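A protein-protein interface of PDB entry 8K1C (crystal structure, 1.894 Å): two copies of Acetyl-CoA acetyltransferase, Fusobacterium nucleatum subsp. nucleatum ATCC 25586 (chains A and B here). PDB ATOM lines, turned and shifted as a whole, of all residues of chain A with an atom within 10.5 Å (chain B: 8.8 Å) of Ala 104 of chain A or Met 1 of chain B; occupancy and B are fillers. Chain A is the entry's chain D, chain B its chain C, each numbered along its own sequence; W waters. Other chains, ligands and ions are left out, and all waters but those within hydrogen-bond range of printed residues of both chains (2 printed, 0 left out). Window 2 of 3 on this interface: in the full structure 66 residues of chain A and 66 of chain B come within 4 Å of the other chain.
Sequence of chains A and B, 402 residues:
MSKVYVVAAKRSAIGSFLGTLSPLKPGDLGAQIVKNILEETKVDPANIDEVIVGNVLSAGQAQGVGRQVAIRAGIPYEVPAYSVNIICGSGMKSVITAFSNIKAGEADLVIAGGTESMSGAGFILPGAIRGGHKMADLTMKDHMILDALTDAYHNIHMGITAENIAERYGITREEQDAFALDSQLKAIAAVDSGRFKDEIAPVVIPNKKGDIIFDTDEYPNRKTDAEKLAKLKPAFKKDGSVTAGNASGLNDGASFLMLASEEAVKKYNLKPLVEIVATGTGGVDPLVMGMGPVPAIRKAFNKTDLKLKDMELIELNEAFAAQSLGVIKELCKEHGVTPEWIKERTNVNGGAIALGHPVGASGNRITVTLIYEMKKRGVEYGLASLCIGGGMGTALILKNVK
The side-chain hydroxyl (OG) of Ser 100 of chain A is in hydrogen-bond range of the side-chain hydroxyl (OG) of Ser 100 of chain B (2.9 Å).
OG of Ser 100 of chain B sits at hydrogen-bond distance from OD1 of Asn 101 of chain A (2.8 Å).
The side-chain amide nitrogen of Asn 101 of chain B is in hydrogen-bond range of the side-chain hydroxyl of Ser 100 of chain A.
NZ of Lys 303 of chain B lies within salt-bridge range of OE2 of Glu 106 of chain A.
The side-chain sulfur of Met 1 of chain B lies close to the backbone carbonyl oxygen of Ala 104 of chain A (3.7 Å).
The side-chain amino group (NZ) of Lys 103 of chain B sits at hydrogen-bond distance from the backbone carbonyl oxygen (O) of Ser 2 of chain B (2.9 Å).
The backbone carbonyl oxygen (O) of Thr 97 of chain B sits close to the side-chain amide nitrogen (ND2) of Asn 101 of chain B (3.3 Å).
The backbone NH (N) of Glu 106 of chain B is in hydrogen-bond range of the backbone carbonyl oxygen (O) of Asn 101 of chain B (2.9 Å).
NZ of Lys 103 of chain A is in hydrogen-bond range of O of Ser 2 of chain A (3.1 Å).
O of Asn 101 of chain A lies within hydrogen-bond range of N of Glu 106 of chain A (2.9 Å).
The backbone NH (N) of Ala 107 of chain A is in hydrogen-bond range of the backbone carbonyl oxygen (O) of Asn 101 of chain A (3.3 Å).
Met 1 of chain A touches Ala 104 of chain B.
Phe 99 of chain A touches Glu 106 of chain B (CD1 to OE2, 3.6 Å).
Ala 104 of chain B touches Ser 100 of chain A.
CB of Ala 104 of chain B touches CB of Lys 103 of chain A (3.8 Å).
Ala 104 of chain A touches Ser 100 of chain B.
Ala 104 of chain A touches Lys 103 of chain B.
Ala 104 of chain A touches Ala 104 of chain B (CB to N, 3.8 Å).
Phe 99 of chain B touches Glu 106 of chain A.
Printed residues of chain B within 4 Å of Met 1 of chain A: Ala 104.
Ala 98 of chain A touches none of the printed residues of chain B.
Of the printed residues of chain B, Phe 99 of chain A touches Glu 106 (3.6 Å).
Of chain A, only Ala 104 (3.7 Å) comes within 4 Å of Met 1 of chain B.
No residue of chain A comes within 4 Å of Ser 2 of chain B.
Ala 98 of chain B touches none of the printed residues of chain A.
Printed residues of chain A within 4 Å of Phe 99 of chain B: Glu 106.
Ser 100 of chain B touches just these residues of chain A: Ser 100 (2.9 Å), Asn 101 (2.8 Å) and Ala 104 (3.5 Å).
Ala 104 of chain B touches just these residues of chain A: Met 1 (3.5 Å), Ser 100 (3.6 Å), Lys 103 (3.8 Å) and Ala 104 (3.8 Å).
Printed residues of chain A within 4 Å of Glu 106 of chain B: Phe 99.
The nearest residue of chain B that does not touch Ala 104 of chain A is Phe 99 of chain B (5.4 Å).
The nearest residue of chain A that does not touch Met 1 of chain B is Lys 103 of chain A (4.4 Å).
Of the 19 printed residues of chain A, 7 touch a printed residue of chain B.
Hydrophobic or aromatic side chains of chain A within 4 Å of the printed part of chain B: Met 1, Phe 99 and Ala 104.
Ser 100 of chain B touches its own counterpart, Ser 100 of chain A.
Ser 100 of chain A touches Asn 101 of chain B, and with the chains exchanged Asn 101 of chain A touches Ser 100 of chain B.
Lys 103 of chain A touches Ala 104 of chain B, and with the chains exchanged Ala 104 of chain A touches Lys 103 of chain B.
Ala 104 of chain B touches its own counterpart, Ala 104 of chain A.
Water W1 bridges the side-chain carboxylate of Glu 106 of chain A and the side-chain amino group of Lys 303 of chain B.
Water W2 bridges the side-chain amide oxygen (OD1) of Asn 101 of chain A (3.1 Å) and the backbone carbonyl oxygen (O) of Ile 96 of chain B (3.5 Å).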
ATOM      1  N   MET A   1      19.164   5.819  28.973  1.00  0.00           N
ATOM      2  CA  MET A   1      19.274   7.274  28.830  1.00  0.00           C
ATOM      3  C   MET A   1      20.118   7.919  29.935  1.00  0.00           C
ATOM      4  O   MET A   1      19.795   7.836  31.122  1.00  0.00           O
ATOM      5  CB  MET A   1      17.880   7.914  28.788  1.00  0.00           C
ATOM      6  CG  MET A   1      17.019   7.435  27.618  1.00  0.00           C
ATOM      7  SD  MET A   1      16.080   8.790  26.882  1.00  0.00           S
ATOM      8  CE  MET A   1      14.974   9.191  28.237  1.00  0.00           C
ATOM      9  N   SER A   2      21.202   8.577  29.520  1.00  0.00           N
ATOM     10  CA  SER A   2      22.152   9.145  30.469  1.00  0.00           C
ATOM     11  C   SER A   2      21.573  10.376  31.154  1.00  0.00           C
ATOM     12  O   SER A   2      20.883  11.186  30.530  1.00  0.00           O
ATOM     13  CB  SER A   2      23.451   9.520  29.752  1.00  0.00           C
ATOM     14  OG  SER A   2      24.239  10.412  30.528  1.00  0.00           O
ATOM     15  N   LYS A   3      21.853  10.504  32.449  1.00  0.00           N
ATOM     16  CA  LYS A   3      21.646  11.758  33.163  1.00  0.00           C
ATOM     17  C   LYS A   3      22.443  12.875  32.490  1.00  0.00           C
ATOM     18  O   LYS A   3      23.437  12.632  31.799  1.00  0.00           O
ATOM     19  CB  LYS A   3      22.091  11.626  34.620  1.00  0.00           C
ATOM     20  CG  LYS A   3      21.352  10.584  35.444  1.00  0.00           C
ATOM     21  CD  LYS A   3      21.842  10.629  36.886  1.00  0.00           C
ATOM     22  CE  LYS A   3      20.874   9.962  37.842  1.00  0.00           C
ATOM     23  NZ  LYS A   3      20.756   8.505  37.570  1.00  0.00           N
ATOM     24  N   VAL A   4      22.005  14.113  32.699  1.00  0.00           N
ATOM     25  CA  VAL A   4      22.635  15.289  32.094  1.00  0.00           C
ATOM     26  C   VAL A   4      23.213  16.142  33.216  1.00  0.00           C
ATOM     27  O   VAL A   4      22.474  16.612  34.093  1.00  0.00           O
ATOM     28  CB  VAL A   4      21.649  16.111  31.244  1.00  0.00           C
ATOM     29  CG1 VAL A   4      22.339  17.371  30.728  1.00  0.00           C
ATOM     30  CG2 VAL A   4      21.075  15.276  30.097  1.00  0.00           C
ATOM     31  N   ILE A  96      18.232  23.357  27.074  1.00  0.00           N
ATOM     32  CA  ILE A  96      17.173  22.361  26.968  1.00  0.00           C
ATOM     33  C   ILE A  96      17.432  21.444  25.779  1.00  0.00           C
ATOM     34  O   ILE A  96      17.279  20.220  25.878  1.00  0.00           O
ATOM     35  CB  ILE A  96      15.804  23.058  26.872  1.00  0.00           C
ATOM     36  CG1 ILE A  96      15.458  23.742  28.201  1.00  0.00           C
ATOM     37  CG2 ILE A  96      14.729  22.070  26.439  1.00  0.00           C
ATOM     38  CD1 ILE A  96      14.052  24.316  28.245  1.00  0.00           C
ATOM     39  N   THR A  97      17.850  22.019  24.647  1.00  0.00           N
ATOM     40  CA  THR A  97      18.197  21.223  23.469  1.00  0.00           C
ATOM     41  C   THR A  97      19.435  20.356  23.712  1.00  0.00           C
ATOM     42  O   THR A  97      19.465  19.182  23.313  1.00  0.00           O
ATOM     43  CB  THR A  97      18.413  22.155  22.277  1.00  0.00           C
ATOM     44  OG1 THR A  97      17.184  22.822  21.982  1.00  0.00           O
ATOM     45  CG2 THR A  97      18.878  21.377  21.034  1.00  0.00           C
ATOM     46  N   ALA A  98      20.465  20.902  24.369  1.00  0.00           N
ATOM     47  CA  ALA A  98      21.612  20.069  24.736  1.00  0.00           C
ATOM     48  C   ALA A  98      21.185  18.916  25.642  1.00  0.00           C
ATOM     49  O   ALA A  98      21.664  17.788  25.495  1.00  0.00           O
ATOM     50  CB  ALA A  98      22.694  20.915  25.419  1.00  0.00           C
ATOM     51  N   PHE A  99      20.279  19.190  26.584  1.00  0.00           N
ATOM     52  CA  PHE A  99      19.711  18.150  27.439  1.00  0.00           C
ATOM     53  C   PHE A  99      19.074  17.035  26.610  1.00  0.00           C
ATOM     54  O   PHE A  99      19.259  15.841  26.890  1.00  0.00           O
ATOM     55  CB  PHE A  99      18.684  18.793  28.382  1.00  0.00           C
ATOM     56  CG  PHE A  99      17.864  17.806  29.162  1.00  0.00           C
ATOM     57  CD1 PHE A  99      16.701  17.261  28.620  1.00  0.00           C
ATOM     58  CD2 PHE A  99      18.229  17.456  30.453  1.00  0.00           C
ATOM     59  CE1 PHE A  99      15.934  16.354  29.330  1.00  0.00           C
ATOM     60  CE2 PHE A  99      17.468  16.551  31.181  1.00  0.00           C
ATOM     61  CZ  PHE A  99      16.313  15.995  30.616  1.00  0.00           C
ATOM     62  N   SER A 100      18.280  17.413  25.609  1.00  0.00           N
ATOM     63  CA  SER A 100      17.644  16.439  24.731  1.00  0.00           C
ATOM     64  C   SER A 100      18.679  15.660  23.920  1.00  0.00           C
ATOM     65  O   SER A 100      18.573  14.435  23.776  1.00  0.00           O
ATOM     66  CB  SER A 100      16.656  17.162  23.814  1.00  0.00           C
ATOM     67  OG  SER A 100      16.233  16.321  22.764  1.00  0.00           O
ATOM     68  N   ASN A 101      19.698  16.347  23.395  1.00  0.00           N
ATOM     69  CA  ASN A 101      20.724  15.668  22.601  1.00  0.00           C
ATOM     70  C   ASN A 101      21.473  14.632  23.429  1.00  0.00           C
ATOM     71  O   ASN A 101      21.767  13.535  22.943  1.00  0.00           O
ATOM     72  CB  ASN A 101      21.703  16.684  22.020  1.00  0.00           C
ATOM     73  CG  ASN A 101      21.069  17.561  20.965  1.00  0.00           C
ATOM     74  OD1 ASN A 101      20.019  17.225  20.407  1.00  0.00           O
ATOM     75  ND2 ASN A 101      21.707  18.676  20.671  1.00  0.00           N
ATOM     76  N   ILE A 102      21.794  14.960  24.685  1.00  0.00           N
ATOM     77  CA  ILE A 102      22.502  14.008  25.534  1.00  0.00           C
ATOM     78  C   ILE A 102      21.583  12.849  25.903  1.00  0.00           C
ATOM     79  O   ILE A 102      21.970  11.676  25.816  1.00  0.00           O
ATOM     80  CB  ILE A 102      23.082  14.725  26.768  1.00  0.00           C
ATOM     81  CG1 ILE A 102      24.256  15.618  26.346  1.00  0.00           C
ATOM     82  CG2 ILE A 102      23.551  13.719  27.825  1.00  0.00           C
ATOM     83  CD1 ILE A 102      24.746  16.581  27.425  1.00  0.00           C
ATOM     84  N   LYS A 103      20.334  13.156  26.260  1.00  0.00           N
ATOM     85  CA  LYS A 103      19.368  12.122  26.615  1.00  0.00           C
ATOM     86  C   LYS A 103      19.136  11.157  25.456  1.00  0.00           C
ATOM     87  O   LYS A 103      19.012   9.943  25.663  1.00  0.00           O
ATOM     88  CB  LYS A 103      18.052  12.781  27.040  1.00  0.00           C
ATOM     89  CG  LYS A 103      17.419  12.205  28.282  1.00  0.00           C
ATOM     90  CD  LYS A 103      17.988  12.838  29.530  1.00  0.00           C
ATOM     91  CE  LYS A 103      17.616  12.006  30.752  1.00  0.00           C
ATOM     92  NZ  LYS A 103      18.400  12.369  31.969  1.00  0.00           N
ATOM     93  N   ALA A 104      19.072  11.677  24.232  1.00  0.00           N
ATOM     94  CA  ALA A 104      18.790  10.865  23.054  1.00  0.00           C
ATOM     95  C   ALA A 104      20.014  10.143  22.509  1.00  0.00           C
ATOM     96  O   ALA A 104      19.893   9.450  21.492  1.00  0.00           O
ATOM     97  CB  ALA A 104      18.191  11.733  21.946  1.00  0.00           C
ATOM     98  N   GLY A 105      21.179  10.283  23.140  1.00  0.00           N
ATOM     99  CA  GLY A 105      22.370   9.635  22.627  1.00  0.00           C
ATOM    100  C   GLY A 105      22.972  10.279  21.399  1.00  0.00           C
ATOM    101  O   GLY A 105      23.805   9.658  20.734  1.00  0.00           O
ATOM    102  N   GLU A 106      22.585  11.510  21.076  1.00  0.00           N
ATOM    103  CA  GLU A 106      23.150  12.227  19.941  1.00  0.00           C
ATOM    104  C   GLU A 106      24.369  13.065  20.308  1.00  0.00           C
ATOM    105  O   GLU A 106      24.977  13.659  19.413  1.00  0.00           O
ATOM    106  CB  GLU A 106      22.084  13.132  19.303  1.00  0.00           C
ATOM    107  CG  GLU A 106      20.912  12.380  18.683  1.00  0.00           C
ATOM    108  CD  GLU A 106      21.096  12.114  17.189  1.00  0.00           C
ATOM    109  OE1 GLU A 106      20.734  12.987  16.350  1.00  0.00           O
ATOM    110  OE2 GLU A 106      21.603  11.020  16.865  1.00  0.00           O
ATOM    111  N   ALA A 107      24.736  13.141  21.587  1.00  0.00           N
ATOM    112  CA  ALA A 107      25.876  13.944  22.015  1.00  0.00           C
ATOM    113  C   ALA A 107      26.259  13.568  23.439  1.00  0.00           C
ATOM    114  O   ALA A 107      25.438  13.069  24.212  1.00  0.00           O
ATOM    115  CB  ALA A 107      25.584  15.444  21.941  1.00  0.00           C
ATOM    116  N   ASP A 108      27.520  13.858  23.775  1.00  0.00           N
ATOM    117  CA  ASP A 108      28.091  13.589  25.085  1.00  0.00           C
ATOM    118  C   ASP A 108      28.636  14.825  25.791  1.00  0.00           C
ATOM    119  O   ASP A 108      28.762  14.800  27.021  1.00  0.00           O
ATOM    120  CB  ASP A 108      29.236  12.573  24.970  1.00  0.00           C
ATOM    121  CG  ASP A 108      28.746  11.179  24.688  1.00  0.00           C
ATOM    122  OD1 ASP A 108      27.984  10.631  25.508  1.00  0.00           O
ATOM    123  OD2 ASP A 108      29.125  10.632  23.640  1.00  0.00           O
ATOM    124  N   VAL A 110      28.446  19.192  25.447  1.00  0.00           N
ATOM    125  CA  VAL A 110      27.829  20.300  24.715  1.00  0.00           C
ATOM    126  C   VAL A 110      28.029  21.597  25.494  1.00  0.00           C
ATOM    127  O   VAL A 110      27.857  21.634  26.721  1.00  0.00           O
ATOM    128  CB  VAL A 110      26.320  20.050  24.466  1.00  0.00           C
ATOM    129  CG1 VAL A 110      25.760  21.087  23.494  1.00  0.00           C
ATOM    130  CG2 VAL A 110      26.066  18.645  23.931  1.00  0.00           C
ATOM    131  N   SER A 261      27.361  14.040  29.411  1.00  0.00           N
ATOM    132  CA  SER A 261      26.757  12.746  29.663  1.00  0.00           C
ATOM    133  C   SER A 261      27.461  12.087  30.847  1.00  0.00           C
ATOM    134  O   SER A 261      28.425  12.624  31.399  1.00  0.00           O
ATOM    135  CB  SER A 261      26.828  11.907  28.384  1.00  0.00           C
ATOM    136  OG  SER A 261      28.116  11.325  28.235  1.00  0.00           O
ATOM    137  N   MET B   1      13.891   3.755  23.082  1.00  0.00           N
ATOM    138  CA  MET B   1      13.668   5.014  22.378  1.00  0.00           C
ATOM    139  C   MET B   1      12.792   4.800  21.135  1.00  0.00           C
ATOM    140  O   MET B   1      12.889   3.770  20.465  1.00  0.00           O
ATOM    141  CB  MET B   1      15.007   5.660  22.004  1.00  0.00           C
ATOM    142  CG  MET B   1      15.850   6.071  23.208  1.00  0.00           C
ATOM    143  SD  MET B   1      17.219   7.185  22.794  1.00  0.00           S
ATOM    144  CE  MET B   1      18.115   6.169  21.609  1.00  0.00           C
ATOM    145  N   SER B   2      11.937   5.775  20.832  1.00  0.00           N
ATOM    146  CA  SER B   2      11.003   5.653  19.720  1.00  0.00           C
ATOM    147  C   SER B   2      11.690   5.833  18.372  1.00  0.00           C
ATOM    148  O   SER B   2      12.665   6.577  18.243  1.00  0.00           O
ATOM    149  CB  SER B   2       9.899   6.695  19.833  1.00  0.00           C
ATOM    150  OG  SER B   2       9.083   6.693  18.662  1.00  0.00           O
ATOM    151  N   LYS B   3      11.148   5.162  17.357  1.00  0.00           N
ATOM    152  CA  LYS B   3      11.478   5.511  15.983  1.00  0.00           C
ATOM    153  C   LYS B   3      10.878   6.874  15.650  1.00  0.00           C
ATOM    154  O   LYS B   3       9.883   7.297  16.248  1.00  0.00           O
ATOM    155  CB  LYS B   3      10.958   4.451  15.013  1.00  0.00           C
ATOM    156  CG  LYS B   3      11.704   3.130  15.089  1.00  0.00           C
ATOM    157  CD  LYS B   3      11.301   2.199  13.958  1.00  0.00           C
ATOM    158  CE  LYS B   3      12.425   1.222  13.672  1.00  0.00           C
ATOM    159  NZ  LYS B   3      12.410   0.714  12.279  1.00  0.00           N
ATOM    160  N   VAL B   4      11.499   7.571  14.701  1.00  0.00           N
ATOM    161  CA  VAL B   4      11.090   8.921  14.313  1.00  0.00           C
ATOM    162  C   VAL B   4      10.554   8.875  12.889  1.00  0.00           C
ATOM    163  O   VAL B   4      11.302   8.594  11.943  1.00  0.00           O
ATOM    164  CB  VAL B   4      12.248   9.925  14.429  1.00  0.00           C
ATOM    165  CG1 VAL B   4      11.809  11.295  13.923  1.00  0.00           C
ATOM    166  CG2 VAL B   4      12.746  10.002  15.873  1.00  0.00           C
ATOM    167  N   ILE B  96      16.483  17.743  12.703  1.00  0.00           N
ATOM    168  CA  ILE B  96      17.452  16.980  13.496  1.00  0.00           C
ATOM    169  C   ILE B  96      17.197  17.164  14.988  1.00  0.00           C
ATOM    170  O   ILE B  96      17.292  16.206  15.775  1.00  0.00           O
ATOM    171  CB  ILE B  96      18.884  17.396  13.099  1.00  0.00           C
ATOM    172  CG1 ILE B  96      19.188  16.907  11.682  1.00  0.00           C
ATOM    173  CG2 ILE B  96      19.913  16.876  14.091  1.00  0.00           C
ATOM    174  CD1 ILE B  96      20.561  17.297  11.179  1.00  0.00           C
ATOM    175  N   THR B  97      16.868  18.396  15.402  1.00  0.00           N
ATOM    176  CA  THR B  97      16.478  18.650  16.789  1.00  0.00           C
ATOM    177  C   THR B  97      15.141  17.989  17.135  1.00  0.00           C
ATOM    178  O   THR B  97      14.982  17.413  18.227  1.00  0.00           O
ATOM    179  CB  THR B  97      16.405  20.154  17.029  1.00  0.00           C
ATOM    180  OG1 THR B  97      17.699  20.722  16.827  1.00  0.00           O
ATOM    181  CG2 THR B  97      15.963  20.451  18.455  1.00  0.00           C
ATOM    182  N   ALA B  98      14.164  18.058  16.227  1.00  0.00           N
ATOM    183  CA  ALA B  98      12.914  17.334  16.449  1.00  0.00           C
ATOM    184  C   ALA B  98      13.177  15.841  16.601  1.00  0.00           C
ATOM    185  O   ALA B  98      12.579  15.178  17.461  1.00  0.00           O
ATOM    186  CB  ALA B  98      11.943  17.588  15.297  1.00  0.00           C
ATOM    187  N   PHE B  99      14.080  15.303  15.773  1.00  0.00           N
ATOM    188  CA  PHE B  99      14.482  13.904  15.892  1.00  0.00           C
ATOM    189  C   PHE B  99      15.032  13.618  17.283  1.00  0.00           C
ATOM    190  O   PHE B  99      14.664  12.622  17.924  1.00  0.00           O
ATOM    191  CB  PHE B  99      15.513  13.594  14.805  1.00  0.00           C
ATOM    192  CG  PHE B  99      16.206  12.262  14.948  1.00  0.00           C
ATOM    193  CD1 PHE B  99      17.308  12.119  15.779  1.00  0.00           C
ATOM    194  CD2 PHE B  99      15.796  11.168  14.201  1.00  0.00           C
ATOM    195  CE1 PHE B  99      17.963  10.909  15.896  1.00  0.00           C
ATOM    196  CE2 PHE B  99      16.460   9.939  14.304  1.00  0.00           C
ATOM    197  CZ  PHE B  99      17.544   9.815  15.159  1.00  0.00           C
ATOM    198  N   SER B 100      15.923  14.487  17.766  1.00  0.00           N
ATOM    199  CA  SER B 100      16.461  14.352  19.119  1.00  0.00           C
ATOM    200  C   SER B 100      15.366  14.401  20.177  1.00  0.00           C
ATOM    201  O   SER B 100      15.345  13.573  21.103  1.00  0.00           O
ATOM    202  CB  SER B 100      17.496  15.445  19.381  1.00  0.00           C
ATOM    203  OG  SER B 100      18.027  15.307  20.689  1.00  0.00           O
ATOM    204  N   ASN B 101      14.479  15.395  20.079  1.00  0.00           N
ATOM    205  CA  ASN B 101      13.427  15.556  21.084  1.00  0.00           C
ATOM    206  C   ASN B 101      12.567  14.298  21.186  1.00  0.00           C
ATOM    207  O   ASN B 101      12.280  13.819  22.290  1.00  0.00           O
ATOM    208  CB  ASN B 101      12.552  16.777  20.762  1.00  0.00           C
ATOM    209  CG  ASN B 101      13.322  18.107  20.804  1.00  0.00           C
ATOM    210  OD1 ASN B 101      12.868  19.116  20.258  1.00  0.00           O
ATOM    211  ND2 ASN B 101      14.472  18.112  21.456  1.00  0.00           N
ATOM    212  N   ILE B 102      12.185  13.721  20.045  1.00  0.00           N
ATOM    213  CA  ILE B 102      11.342  12.524  20.064  1.00  0.00           C
ATOM    214  C   ILE B 102      12.097  11.333  20.668  1.00  0.00           C
ATOM    215  O   ILE B 102      11.560  10.613  21.519  1.00  0.00           O
ATOM    216  CB  ILE B 102      10.810  12.222  18.648  1.00  0.00           C
ATOM    217  CG1 ILE B 102       9.667  13.187  18.315  1.00  0.00           C
ATOM    218  CG2 ILE B 102      10.348  10.752  18.528  1.00  0.00           C
ATOM    219  CD1 ILE B 102       9.399  13.384  16.820  1.00  0.00           C
ATOM    220  N   LYS B 103      13.356  11.123  20.259  1.00  0.00           N
ATOM    221  CA  LYS B 103      14.144  10.019  20.816  1.00  0.00           C
ATOM    222  C   LYS B 103      14.333  10.170  22.316  1.00  0.00           C
ATOM    223  O   LYS B 103      14.348   9.173  23.053  1.00  0.00           O
ATOM    224  CB  LYS B 103      15.514   9.935  20.142  1.00  0.00           C
ATOM    225  CG  LYS B 103      15.479   9.598  18.670  1.00  0.00           C
ATOM    226  CD  LYS B 103      15.749   8.130  18.417  1.00  0.00           C
ATOM    227  CE  LYS B 103      15.383   7.758  16.985  1.00  0.00           C
ATOM    228  NZ  LYS B 103      15.121   6.288  16.823  1.00  0.00           N
ATOM    229  N   ALA B 104      14.498  11.407  22.787  1.00  0.00           N
ATOM    230  CA  ALA B 104      14.683  11.654  24.211  1.00  0.00           C
ATOM    231  C   ALA B 104      13.388  11.574  25.006  1.00  0.00           C
ATOM    232  O   ALA B 104      13.439  11.593  26.241  1.00  0.00           O
ATOM    233  CB  ALA B 104      15.329  13.026  24.424  1.00  0.00           C
ATOM    234  N   GLY B 105      12.241  11.501  24.344  1.00  0.00           N
ATOM    235  CA  GLY B 105      10.972  11.518  25.042  1.00  0.00           C
ATOM    236  C   GLY B 105      10.514  12.890  25.467  1.00  0.00           C
ATOM    237  O   GLY B 105       9.571  13.000  26.258  1.00  0.00           O
ATOM    238  N   GLU B 106      11.169  13.937  24.973  1.00  0.00           N
ATOM    239  CA  GLU B 106      10.776  15.313  25.218  1.00  0.00           C
ATOM    240  C   GLU B 106       9.605  15.756  24.348  1.00  0.00           C
ATOM    241  O   GLU B 106       8.982  16.776  24.645  1.00  0.00           O
ATOM    242  CB  GLU B 106      11.977  16.226  24.964  1.00  0.00           C
ATOM    243  CG  GLU B 106      13.132  16.006  25.927  1.00  0.00           C
ATOM    244  CD  GLU B 106      12.958  16.799  27.202  1.00  0.00           C
ATOM    245  OE1 GLU B 106      12.285  16.271  28.106  1.00  0.00           O
ATOM    246  OE2 GLU B 106      13.474  17.953  27.289  1.00  0.00           O
ATOM    247  N   SER B 261       6.421  10.418  16.957  1.00  0.00           N
ATOM    248  CA  SER B 261       6.821   9.204  17.659  1.00  0.00           C
ATOM    249  C   SER B 261       5.938   8.027  17.228  1.00  0.00           C
ATOM    250  O   SER B 261       5.007   8.166  16.425  1.00  0.00           O
ATOM    251  CB  SER B 261       6.727   9.433  19.166  1.00  0.00           C
ATOM    252  OG  SER B 261       5.361   9.489  19.560  1.00  0.00           O
ATOM    253  N   GLU B 262       6.213   6.842  17.783  1.00  0.00           N
ATOM    254  CA  GLU B 262       5.337   5.709  17.496  1.00  0.00           C
ATOM    255  C   GLU B 262       3.991   5.842  18.208  1.00  0.00           C
ATOM    256  O   GLU B 262       2.952   5.495  17.629  1.00  0.00           O
ATOM    257  CB  GLU B 262       6.034   4.391  17.842  1.00  0.00           C
ATOM    258  CG  GLU B 262       7.109   4.036  16.821  1.00  0.00           C
ATOM    259  CD  GLU B 262       8.163   3.070  17.339  1.00  0.00           C
ATOM    260  OE1 GLU B 262       8.810   3.363  18.368  1.00  0.00           O
ATOM    261  OE2 GLU B 262       8.377   2.029  16.680  1.00  0.00           O
ATOM    262  N   GLU B 263       3.978   6.358  19.452  1.00  0.00           N
ATOM    263  CA  GLU B 263       2.711   6.635  20.134  1.00  0.00           C
ATOM    264  C   GLU B 263       1.852   7.588  19.326  1.00  0.00           C
ATOM    265  O   GLU B 263       0.643   7.377  19.171  1.00  0.00           O
ATOM    266  CB  GLU B 263       2.930   7.240  21.526  1.00  0.00           C
ATOM    267  CG  GLU B 263       3.686   6.409  22.546  1.00  0.00           C
ATOM    268  CD  GLU B 263       5.189   6.394  22.300  1.00  0.00           C
ATOM    269  OE1 GLU B 263       5.739   5.327  21.941  1.00  0.00           O
ATOM    270  OE2 GLU B 263       5.838   7.467  22.430  1.00  0.00           O
ATOM    271  N   GLU B 275      10.818   6.964   7.469  1.00  0.00           N
ATOM    272  CA  GLU B 275      11.436   6.993   8.785  1.00  0.00           C
ATOM    273  C   GLU B 275      12.795   7.672   8.686  1.00  0.00           C
ATOM    274  O   GLU B 275      13.531   7.461   7.713  1.00  0.00           O
ATOM    275  CB  GLU B 275      11.600   5.573   9.340  1.00  0.00           C
ATOM    276  CG  GLU B 275      12.340   5.516  10.657  1.00  0.00           C
ATOM    277  CD  GLU B 275      12.721   4.109  11.038  1.00  0.00           C
ATOM    278  OE1 GLU B 275      12.220   3.157  10.397  1.00  0.00           O
ATOM    279  OE2 GLU B 275      13.511   3.956  11.991  1.00  0.00           O
ATOM    280  N   LYS B 303      26.566   5.965  12.548  1.00  0.00           N
ATOM    281  CA  LYS B 303      25.550   5.587  13.525  1.00  0.00           C
ATOM    282  C   LYS B 303      24.681   4.420  13.065  1.00  0.00           C
ATOM    283  O   LYS B 303      23.723   4.072  13.760  1.00  0.00           O
ATOM    284  CB  LYS B 303      24.639   6.782  13.850  1.00  0.00           C
ATOM    285  CG  LYS B 303      25.341   7.974  14.468  1.00  0.00           C
ATOM    286  CD  LYS B 303      24.338   9.054  14.849  1.00  0.00           C
ATOM    287  CE  LYS B 303      24.921  10.442  14.652  1.00  0.00           C
ATOM    288  NZ  LYS B 303      23.938  11.499  15.022  1.00  0.00           N
HETATM  289  O   HOH W   1      21.042   9.892  14.389  1.00  0.00           O
HETATM  290  O   HOH W   2      20.349  16.431  17.442  1.00  0.00           O
